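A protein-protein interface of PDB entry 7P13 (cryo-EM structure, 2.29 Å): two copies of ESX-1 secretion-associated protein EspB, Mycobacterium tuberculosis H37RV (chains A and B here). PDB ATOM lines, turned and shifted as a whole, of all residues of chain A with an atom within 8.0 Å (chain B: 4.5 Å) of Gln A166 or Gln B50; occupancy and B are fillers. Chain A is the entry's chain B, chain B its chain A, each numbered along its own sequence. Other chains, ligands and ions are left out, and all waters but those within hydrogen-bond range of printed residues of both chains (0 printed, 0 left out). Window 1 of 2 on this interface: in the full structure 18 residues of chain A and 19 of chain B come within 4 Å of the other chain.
The side-chain amide nitrogen (NE2) of Gln B50 sits close to the side-chain amide nitrogen (NE2) of Gln A166 (3.1 Å).
OG of Ser B54 sits at hydrogen-bond distance from O of Gln B50 (3.4 Å).
NE2 of Gln A166 is in hydrogen-bond range of OD1 of Asn A162 (2.7 Å).
CB of Asn A159 touches ND2 of Asn B46, at 3.8 Å.
Asn B46 touches Leu A163 (OD1 to CD1, 3.8 Å).
CD1 of Leu A163 touches CG of Gln B49, at 3.6 Å.
O of Leu A163 touches CD1 of Leu B53, 3.7 Å away.
Leu B53 touches Gln A166.
Gln A166 touches Pro B274.
Gly A167 touches Leu B53.
Of the printed residues of chain B, Asn A159 touches Asn B46.
Asn A162 touches none of the printed residues of chain B.
Of the printed residues of chain B, Gln A166 touches Gln B50, Leu B53 and Pro B274.
Printed residues of chain B within 4 Å of Gly A167: Leu B53.
Of the printed residues of chain A, Gln B50 touches Gln A166.
Of the printed residues of chain A, Leu B53 touches Leu A163 (3.7 Å), Gln A166 (3.9 Å) and Gly A167 (3.6 Å).
Printed residues of chain A within 4 Å of Pro B274: Gln A166 (3.2 Å).
The nearest printed residue of chain B that does not touch Gln A166 is Ser B54 (5.5 Å).
The nearest printed residue of chain A that does not touch Leu B53 is Asn A162 (5.7 Å).
Hydrophobic or aromatic side chains of chain B within 4 Å of the printed part of chain A: Leu B53 and Pro B274.
Of the 20 printed residues of chain A, 4 touch a printed residue of chain B.
Among the printed residues, no Asp or Glu carboxylate lies within 4 Å of a Lys or Arg side-chain nitrogen of the other chain.
No position is printed for both chains.
Of the 8 pairs that touch across the chains among the printed residues, none has its exchanged pair printed and touching as well.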
ATOM      1  N   ASN A 159      17.966  23.922 -13.302  1.00  0.00           N
ATOM      2  CA  ASN A 159      16.792  23.818 -12.444  1.00  0.00           C
ATOM      3  C   ASN A 159      16.128  25.175 -12.262  1.00  0.00           C
ATOM      4  O   ASN A 159      14.890  25.294 -12.292  1.00  0.00           O
ATOM      5  CB  ASN A 159      17.187  23.241 -11.093  1.00  0.00           C
ATOM      6  CG  ASN A 159      17.167  21.749 -11.077  1.00  0.00           C
ATOM      7  OD1 ASN A 159      16.385  21.128 -11.773  1.00  0.00           O
ATOM      8  ND2 ASN A 159      18.033  21.159 -10.286  1.00  0.00           N
ATOM      9  N   THR A 160      16.943  26.211 -12.091  1.00  0.00           N
ATOM     10  CA  THR A 160      16.412  27.556 -12.021  1.00  0.00           C
ATOM     11  C   THR A 160      15.705  27.925 -13.308  1.00  0.00           C
ATOM     12  O   THR A 160      14.651  28.559 -13.280  1.00  0.00           O
ATOM     13  CB  THR A 160      17.522  28.549 -11.721  1.00  0.00           C
ATOM     14  OG1 THR A 160      18.009  28.317 -10.409  1.00  0.00           O
ATOM     15  CG2 THR A 160      16.995  29.925 -11.788  1.00  0.00           C
ATOM     16  N   PHE A 161      16.253  27.512 -14.439  1.00  0.00           N
ATOM     17  CA  PHE A 161      15.601  27.815 -15.698  1.00  0.00           C
ATOM     18  C   PHE A 161      14.272  27.095 -15.853  1.00  0.00           C
ATOM     19  O   PHE A 161      13.358  27.638 -16.467  1.00  0.00           O
ATOM     20  CB  PHE A 161      16.502  27.470 -16.864  1.00  0.00           C
ATOM     21  CG  PHE A 161      16.051  28.060 -18.140  1.00  0.00           C
ATOM     22  CD1 PHE A 161      16.071  29.426 -18.321  1.00  0.00           C
ATOM     23  CD2 PHE A 161      15.577  27.260 -19.153  1.00  0.00           C
ATOM     24  CE1 PHE A 161      15.650  29.978 -19.492  1.00  0.00           C
ATOM     25  CE2 PHE A 161      15.157  27.803 -20.324  1.00  0.00           C
ATOM     26  CZ  PHE A 161      15.198  29.171 -20.499  1.00  0.00           C
ATOM     27  N   ASN A 162      14.166  25.871 -15.344  1.00  0.00           N
ATOM     28  CA  ASN A 162      12.889  25.165 -15.303  1.00  0.00           C
ATOM     29  C   ASN A 162      11.832  25.984 -14.571  1.00  0.00           C
ATOM     30  O   ASN A 162      10.727  26.209 -15.085  1.00  0.00           O
ATOM     31  CB  ASN A 162      13.087  23.805 -14.635  1.00  0.00           C
ATOM     32  CG  ASN A 162      11.797  23.175 -14.171  1.00  0.00           C
ATOM     33  OD1 ASN A 162      10.795  23.199 -14.862  1.00  0.00           O
ATOM     34  ND2 ASN A 162      11.815  22.624 -12.981  1.00  0.00           N
ATOM     35  N   LEU A 163      12.179  26.472 -13.384  1.00  0.00           N
ATOM     36  CA  LEU A 163      11.230  27.305 -12.650  1.00  0.00           C
ATOM     37  C   LEU A 163      10.930  28.610 -13.381  1.00  0.00           C
ATOM     38  O   LEU A 163       9.781  29.064 -13.411  1.00  0.00           O
ATOM     39  CB  LEU A 163      11.752  27.593 -11.256  1.00  0.00           C
ATOM     40  CG  LEU A 163      11.916  26.342 -10.416  1.00  0.00           C
ATOM     41  CD1 LEU A 163      12.288  26.711  -9.013  1.00  0.00           C
ATOM     42  CD2 LEU A 163      10.653  25.520 -10.440  1.00  0.00           C
ATOM     43  N   THR A 164      11.946  29.212 -13.986  1.00  0.00           N
ATOM     44  CA  THR A 164      11.765  30.467 -14.695  1.00  0.00           C
ATOM     45  C   THR A 164      10.834  30.307 -15.885  1.00  0.00           C
ATOM     46  O   THR A 164       9.987  31.163 -16.130  1.00  0.00           O
ATOM     47  CB  THR A 164      13.115  30.996 -15.157  1.00  0.00           C
ATOM     48  OG1 THR A 164      13.933  31.257 -14.026  1.00  0.00           O
ATOM     49  CG2 THR A 164      12.946  32.251 -15.934  1.00  0.00           C
ATOM     50  N   LEU A 165      10.994  29.227 -16.638  1.00  0.00           N
ATOM     51  CA  LEU A 165      10.124  28.962 -17.769  1.00  0.00           C
ATOM     52  C   LEU A 165       8.690  28.762 -17.328  1.00  0.00           C
ATOM     53  O   LEU A 165       7.775  29.303 -17.945  1.00  0.00           O
ATOM     54  CB  LEU A 165      10.609  27.732 -18.514  1.00  0.00           C
ATOM     55  CG  LEU A 165      11.757  27.867 -19.501  1.00  0.00           C
ATOM     56  CD1 LEU A 165      11.969  26.531 -20.178  1.00  0.00           C
ATOM     57  CD2 LEU A 165      11.465  28.947 -20.506  1.00  0.00           C
ATOM     58  N   GLN A 166       8.474  27.993 -16.257  1.00  0.00           N
ATOM     59  CA  GLN A 166       7.114  27.821 -15.758  1.00  0.00           C
ATOM     60  C   GLN A 166       6.508  29.127 -15.278  1.00  0.00           C
ATOM     61  O   GLN A 166       5.293  29.299 -15.327  1.00  0.00           O
ATOM     62  CB  GLN A 166       7.077  26.816 -14.623  1.00  0.00           C
ATOM     63  CG  GLN A 166       7.389  25.429 -15.018  1.00  0.00           C
ATOM     64  CD  GLN A 166       7.402  24.514 -13.840  1.00  0.00           C
ATOM     65  OE1 GLN A 166       6.375  24.274 -13.237  1.00  0.00           O
ATOM     66  NE2 GLN A 166       8.565  24.005 -13.493  1.00  0.00           N
ATOM     67  N   GLY A 167       7.328  30.056 -14.808  1.00  0.00           N
ATOM     68  CA  GLY A 167       6.769  31.315 -14.379  1.00  0.00           C
ATOM     69  C   GLY A 167       6.342  32.234 -15.497  1.00  0.00           C
ATOM     70  O   GLY A 167       5.629  33.198 -15.241  1.00  0.00           O
ATOM     71  N   ASP A 168       6.819  32.017 -16.706  1.00  0.00           N
ATOM     72  CA  ASP A 168       6.509  32.914 -17.811  1.00  0.00           C
ATOM     73  C   ASP A 168       5.516  32.307 -18.803  1.00  0.00           C
ATOM     74  O   ASP A 168       5.799  32.203 -19.975  1.00  0.00           O
ATOM     75  CB  ASP A 168       7.793  33.320 -18.506  1.00  0.00           C
ATOM     76  CG  ASP A 168       7.633  34.558 -19.323  1.00  0.00           C
ATOM     77  OD1 ASP A 168       6.616  35.241 -19.168  1.00  0.00           O
ATOM     78  OD2 ASP A 168       8.518  34.852 -20.135  1.00  0.00           O
ATOM     79  N   VAL A 169       4.314  31.966 -18.374  1.00  0.00           N
ATOM     80  CA  VAL A 169       3.367  31.441 -19.350  1.00  0.00           C
ATOM     81  C   VAL A 169       2.027  32.139 -19.285  1.00  0.00           C
ATOM     82  O   VAL A 169       1.066  31.682 -19.898  1.00  0.00           O
ATOM     83  CB  VAL A 169       3.151  29.926 -19.195  1.00  0.00           C
ATOM     84  CG1 VAL A 169       4.436  29.189 -19.408  1.00  0.00           C
ATOM     85  CG2 VAL A 169       2.556  29.608 -17.860  1.00  0.00           C
ATOM     86  N   LYS A 170       1.943  33.251 -18.567  1.00  0.00           N
ATOM     87  CA  LYS A 170       0.724  34.037 -18.631  1.00  0.00           C
ATOM     88  C   LYS A 170       0.504  34.625 -20.006  1.00  0.00           C
ATOM     89  O   LYS A 170      -0.638  34.876 -20.378  1.00  0.00           O
ATOM     90  CB  LYS A 170       0.740  35.158 -17.614  1.00  0.00           C
ATOM     91  CG  LYS A 170       0.695  34.694 -16.222  1.00  0.00           C
ATOM     92  CD  LYS A 170      -0.453  33.770 -15.979  1.00  0.00           C
ATOM     93  CE  LYS A 170      -0.529  33.434 -14.507  1.00  0.00           C
ATOM     94  NZ  LYS A 170      -1.778  32.712 -14.155  1.00  0.00           N
ATOM     95  N   ARG A 194       2.138  27.145 -25.101  1.00  0.00           N
ATOM     96  CA  ARG A 194       2.256  26.893 -23.673  1.00  0.00           C
ATOM     97  C   ARG A 194       2.679  25.456 -23.380  1.00  0.00           C
ATOM     98  O   ARG A 194       3.547  25.223 -22.533  1.00  0.00           O
ATOM     99  CB  ARG A 194       0.941  27.203 -22.984  1.00  0.00           C
ATOM    100  CG  ARG A 194       1.022  27.208 -21.495  1.00  0.00           C
ATOM    101  CD  ARG A 194      -0.323  26.959 -20.914  1.00  0.00           C
ATOM    102  NE  ARG A 194      -0.282  26.870 -19.465  1.00  0.00           N
ATOM    103  CZ  ARG A 194      -0.556  27.878 -18.650  1.00  0.00           C
ATOM    104  NH1 ARG A 194      -0.898  29.052 -19.133  1.00  0.00           N
ATOM    105  NH2 ARG A 194      -0.487  27.706 -17.349  1.00  0.00           N
ATOM    106  N   ILE A 197       6.313  24.988 -24.166  1.00  0.00           N
ATOM    107  CA  ILE A 197       7.181  25.603 -23.175  1.00  0.00           C
ATOM    108  C   ILE A 197       7.231  24.770 -21.900  1.00  0.00           C
ATOM    109  O   ILE A 197       8.288  24.628 -21.283  1.00  0.00           O
ATOM    110  CB  ILE A 197       6.731  27.046 -22.900  1.00  0.00           C
ATOM    111  CG1 ILE A 197       7.121  27.947 -24.057  1.00  0.00           C
ATOM    112  CG2 ILE A 197       7.347  27.560 -21.629  1.00  0.00           C
ATOM    113  CD1 ILE A 197       8.556  28.265 -24.104  1.00  0.00           C
ATOM    114  N   LEU A 198       6.101  24.209 -21.484  1.00  0.00           N
ATOM    115  CA  LEU A 198       6.097  23.358 -20.303  1.00  0.00           C
ATOM    116  C   LEU A 198       6.927  22.106 -20.523  1.00  0.00           C
ATOM    117  O   LEU A 198       7.646  21.660 -19.624  1.00  0.00           O
ATOM    118  CB  LEU A 198       4.672  22.996 -19.922  1.00  0.00           C
ATOM    119  CG  LEU A 198       3.921  24.155 -19.284  1.00  0.00           C
ATOM    120  CD1 LEU A 198       2.537  23.753 -18.879  1.00  0.00           C
ATOM    121  CD2 LEU A 198       4.668  24.699 -18.104  1.00  0.00           C
ATOM    122  N   HIS A 199       6.857  21.539 -21.721  1.00  0.00           N
ATOM    123  CA  HIS A 199       7.690  20.392 -22.032  1.00  0.00           C
ATOM    124  C   HIS A 199       9.167  20.761 -22.010  1.00  0.00           C
ATOM    125  O   HIS A 199      10.002  19.978 -21.556  1.00  0.00           O
ATOM    126  CB  HIS A 199       7.292  19.817 -23.381  1.00  0.00           C
ATOM    127  CG  HIS A 199       7.925  18.502 -23.683  1.00  0.00           C
ATOM    128  ND1 HIS A 199       8.661  18.276 -24.820  1.00  0.00           N
ATOM    129  CD2 HIS A 199       7.944  17.342 -22.992  1.00  0.00           C
ATOM    130  CE1 HIS A 199       9.091  17.031 -24.826  1.00  0.00           C
ATOM    131  NE2 HIS A 199       8.674  16.444 -23.725  1.00  0.00           N
ATOM    132  N   MET A 200       9.505  21.954 -22.483  1.00  0.00           N
ATOM    133  CA  MET A 200      10.893  22.391 -22.438  1.00  0.00           C
ATOM    134  C   MET A 200      11.376  22.578 -21.006  1.00  0.00           C
ATOM    135  O   MET A 200      12.527  22.275 -20.692  1.00  0.00           O
ATOM    136  CB  MET A 200      11.065  23.679 -23.239  1.00  0.00           C
ATOM    137  CG  MET A 200      10.968  23.507 -24.752  1.00  0.00           C
ATOM    138  SD  MET A 200      12.129  22.324 -25.449  1.00  0.00           S
ATOM    139  CE  MET A 200      13.629  23.284 -25.434  1.00  0.00           C
ATOM    140  N   ALA A 201      10.514  23.078 -20.127  1.00  0.00           N
ATOM    141  CA  ALA A 201      10.875  23.185 -18.720  1.00  0.00           C
ATOM    142  C   ALA A 201      11.129  21.817 -18.110  1.00  0.00           C
ATOM    143  O   ALA A 201      12.082  21.629 -17.344  1.00  0.00           O
ATOM    144  CB  ALA A 201       9.777  23.903 -17.952  1.00  0.00           C
ATOM    145  N   LYS A 202      10.288  20.853 -18.452  1.00  0.00           N
ATOM    146  CA  LYS A 202      10.479  19.493 -17.974  1.00  0.00           C
ATOM    147  C   LYS A 202      11.793  18.901 -18.478  1.00  0.00           C
ATOM    148  O   LYS A 202      12.496  18.202 -17.742  1.00  0.00           O
ATOM    149  CB  LYS A 202       9.298  18.651 -18.414  1.00  0.00           C
ATOM    150  CG  LYS A 202       9.255  17.314 -17.832  1.00  0.00           C
ATOM    151  CD  LYS A 202       8.088  16.546 -18.369  1.00  0.00           C
ATOM    152  CE  LYS A 202       6.805  17.349 -18.296  1.00  0.00           C
ATOM    153  NZ  LYS A 202       6.587  17.955 -16.974  1.00  0.00           N
ATOM    154  N   ALA A 205      14.625  20.285 -16.457  1.00  0.00           N
ATOM    155  CA  ALA A 205      14.736  19.548 -15.211  1.00  0.00           C
ATOM    156  C   ALA A 205      15.423  18.211 -15.418  1.00  0.00           C
ATOM    157  O   ALA A 205      16.249  17.800 -14.601  1.00  0.00           O
ATOM    158  CB  ALA A 205      13.362  19.346 -14.594  1.00  0.00           C
ATOM    159  N   ASN B  46      13.714  25.061  -4.200  1.00  0.00           N
ATOM    160  CA  ASN B  46      13.155  24.777  -5.508  1.00  0.00           C
ATOM    161  C   ASN B  46      11.829  24.046  -5.389  1.00  0.00           C
ATOM    162  O   ASN B  46      10.908  24.306  -6.162  1.00  0.00           O
ATOM    163  CB  ASN B  46      14.152  23.993  -6.337  1.00  0.00           C
ATOM    164  CG  ASN B  46      15.258  24.855  -6.863  1.00  0.00           C
ATOM    165  OD1 ASN B  46      15.248  26.064  -6.695  1.00  0.00           O
ATOM    166  ND2 ASN B  46      16.222  24.241  -7.503  1.00  0.00           N
ATOM    167  N   ALA B  47      11.702  23.151  -4.416  1.00  0.00           N
ATOM    168  CA  ALA B  47      10.427  22.489  -4.190  1.00  0.00           C
ATOM    169  C   ALA B  47       9.353  23.481  -3.777  1.00  0.00           C
ATOM    170  O   ALA B  47       8.210  23.396  -4.238  1.00  0.00           O
ATOM    171  CB  ALA B  47      10.580  21.405  -3.135  1.00  0.00           C
ATOM    172  N   ALA B  48       9.701  24.426  -2.914  1.00  0.00           N
ATOM    173  CA  ALA B  48       8.727  25.430  -2.516  1.00  0.00           C
ATOM    174  C   ALA B  48       8.309  26.298  -3.691  1.00  0.00           C
ATOM    175  O   ALA B  48       7.130  26.621  -3.841  1.00  0.00           O
ATOM    176  CB  ALA B  48       9.281  26.290  -1.388  1.00  0.00           C
ATOM    177  N   GLN B  49       9.258  26.682  -4.533  1.00  0.00           N
ATOM    178  CA  GLN B  49       8.901  27.482  -5.688  1.00  0.00           C
ATOM    179  C   GLN B  49       8.050  26.687  -6.671  1.00  0.00           C
ATOM    180  O   GLN B  49       7.140  27.246  -7.286  1.00  0.00           O
ATOM    181  CB  GLN B  49      10.159  28.034  -6.344  1.00  0.00           C
ATOM    182  CG  GLN B  49       9.919  28.925  -7.532  1.00  0.00           C
ATOM    183  CD  GLN B  49       8.923  30.040  -7.272  1.00  0.00           C
ATOM    184  OE1 GLN B  49       8.683  30.425  -6.142  1.00  0.00           O
ATOM    185  NE2 GLN B  49       8.343  30.561  -8.324  1.00  0.00           N
ATOM    186  N   GLN B  50       8.308  25.387  -6.803  1.00  0.00           N
ATOM    187  CA  GLN B  50       7.468  24.544  -7.641  1.00  0.00           C
ATOM    188  C   GLN B  50       6.047  24.491  -7.111  1.00  0.00           C
ATOM    189  O   GLN B  50       5.090  24.543  -7.883  1.00  0.00           O
ATOM    190  CB  GLN B  50       8.049  23.138  -7.733  1.00  0.00           C
ATOM    191  CG  GLN B  50       7.216  22.148  -8.550  1.00  0.00           C
ATOM    192  CD  GLN B  50       7.022  22.573 -10.000  1.00  0.00           C
ATOM    193  OE1 GLN B  50       5.942  22.973 -10.399  1.00  0.00           O
ATOM    194  NE2 GLN B  50       8.066  22.485 -10.783  1.00  0.00           N
ATOM    195  N   LEU B  51       5.895  24.395  -5.797  1.00  0.00           N
ATOM    196  CA  LEU B  51       4.567  24.400  -5.207  1.00  0.00           C
ATOM    197  C   LEU B  51       3.859  25.726  -5.427  1.00  0.00           C
ATOM    198  O   LEU B  51       2.654  25.753  -5.683  1.00  0.00           O
ATOM    199  CB  LEU B  51       4.654  24.083  -3.725  1.00  0.00           C
ATOM    200  CG  LEU B  51       4.825  22.605  -3.428  1.00  0.00           C
ATOM    201  CD1 LEU B  51       4.914  22.388  -1.956  1.00  0.00           C
ATOM    202  CD2 LEU B  51       3.695  21.793  -4.002  1.00  0.00           C
ATOM    203  N   VAL B  52       4.592  26.830  -5.324  1.00  0.00           N
ATOM    204  CA  VAL B  52       4.011  28.140  -5.585  1.00  0.00           C
ATOM    205  C   VAL B  52       3.503  28.219  -7.018  1.00  0.00           C
ATOM    206  O   VAL B  52       2.385  28.673  -7.275  1.00  0.00           O
ATOM    207  CB  VAL B  52       5.035  29.247  -5.287  1.00  0.00           C
ATOM    208  CG1 VAL B  52       4.623  30.517  -5.936  1.00  0.00           C
ATOM    209  CG2 VAL B  52       5.188  29.446  -3.808  1.00  0.00           C
ATOM    210  N   LEU B  53       4.304  27.736  -7.958  1.00  0.00           N
ATOM    211  CA  LEU B  53       3.911  27.756  -9.358  1.00  0.00           C
ATOM    212  C   LEU B  53       2.706  26.866  -9.627  1.00  0.00           C
ATOM    213  O   LEU B  53       1.807  27.243 -10.383  1.00  0.00           O
ATOM    214  CB  LEU B  53       5.087  27.341 -10.223  1.00  0.00           C
ATOM    215  CG  LEU B  53       6.120  28.450 -10.404  1.00  0.00           C
ATOM    216  CD1 LEU B  53       7.466  27.861 -10.741  1.00  0.00           C
ATOM    217  CD2 LEU B  53       5.689  29.425 -11.458  1.00  0.00           C
ATOM    218  N   SER B  54       2.667  25.684  -9.025  1.00  0.00           N
ATOM    219  CA  SER B  54       1.527  24.802  -9.220  1.00  0.00           C
ATOM    220  C   SER B  54       0.252  25.387  -8.638  1.00  0.00           C
ATOM    221  O   SER B  54      -0.820  25.257  -9.231  1.00  0.00           O
ATOM    222  CB  SER B  54       1.803  23.436  -8.615  1.00  0.00           C
ATOM    223  OG  SER B  54       2.707  22.710  -9.405  1.00  0.00           O
ATOM    224  N   LEU B 272       9.943  17.922  -7.792  1.00  0.00           N
ATOM    225  CA  LEU B 272       8.512  17.717  -7.879  1.00  0.00           C
ATOM    226  C   LEU B 272       8.020  17.915  -9.297  1.00  0.00           C
ATOM    227  O   LEU B 272       8.504  18.788 -10.010  1.00  0.00           O
ATOM    228  CB  LEU B 272       7.783  18.681  -6.971  1.00  0.00           C
ATOM    229  CG  LEU B 272       8.027  18.407  -5.513  1.00  0.00           C
ATOM    230  CD1 LEU B 272       7.447  19.550  -4.714  1.00  0.00           C
ATOM    231  CD2 LEU B 272       7.387  17.110  -5.141  1.00  0.00           C
ATOM    232  N   GLU B 273       7.091  17.136  -9.686  1.00  0.00           N
ATOM    233  CA  GLU B 273       6.457  17.431 -10.953  1.00  0.00           C
ATOM    234  C   GLU B 273       5.554  18.641 -10.814  1.00  0.00           C
ATOM    235  O   GLU B 273       4.861  18.783  -9.815  1.00  0.00           O
ATOM    236  CB  GLU B 273       5.638  16.266 -11.437  1.00  0.00           C
ATOM    237  CG  GLU B 273       6.359  14.982 -11.387  1.00  0.00           C
ATOM    238  CD  GLU B 273       7.522  14.936 -12.321  1.00  0.00           C
ATOM    239  OE1 GLU B 273       7.689  15.856 -13.147  1.00  0.00           O
ATOM    240  OE2 GLU B 273       8.291  13.963 -12.236  1.00  0.00           O
ATOM    241  N   PRO B 274       5.548  19.526 -11.787  1.00  0.00           N
ATOM    242  CA  PRO B 274       4.526  20.563 -11.804  1.00  0.00           C
ATOM    243  C   PRO B 274       3.150  19.954 -11.981  1.00  0.00           C
ATOM    244  O   PRO B 274       2.974  18.937 -12.641  1.00  0.00           O
ATOM    245  CB  PRO B 274       4.919  21.432 -12.998  1.00  0.00           C
ATOM    246  CG  PRO B 274       5.805  20.606 -13.794  1.00  0.00           C
ATOM    247  CD  PRO B 274       6.456  19.611 -12.932  1.00  0.00           C
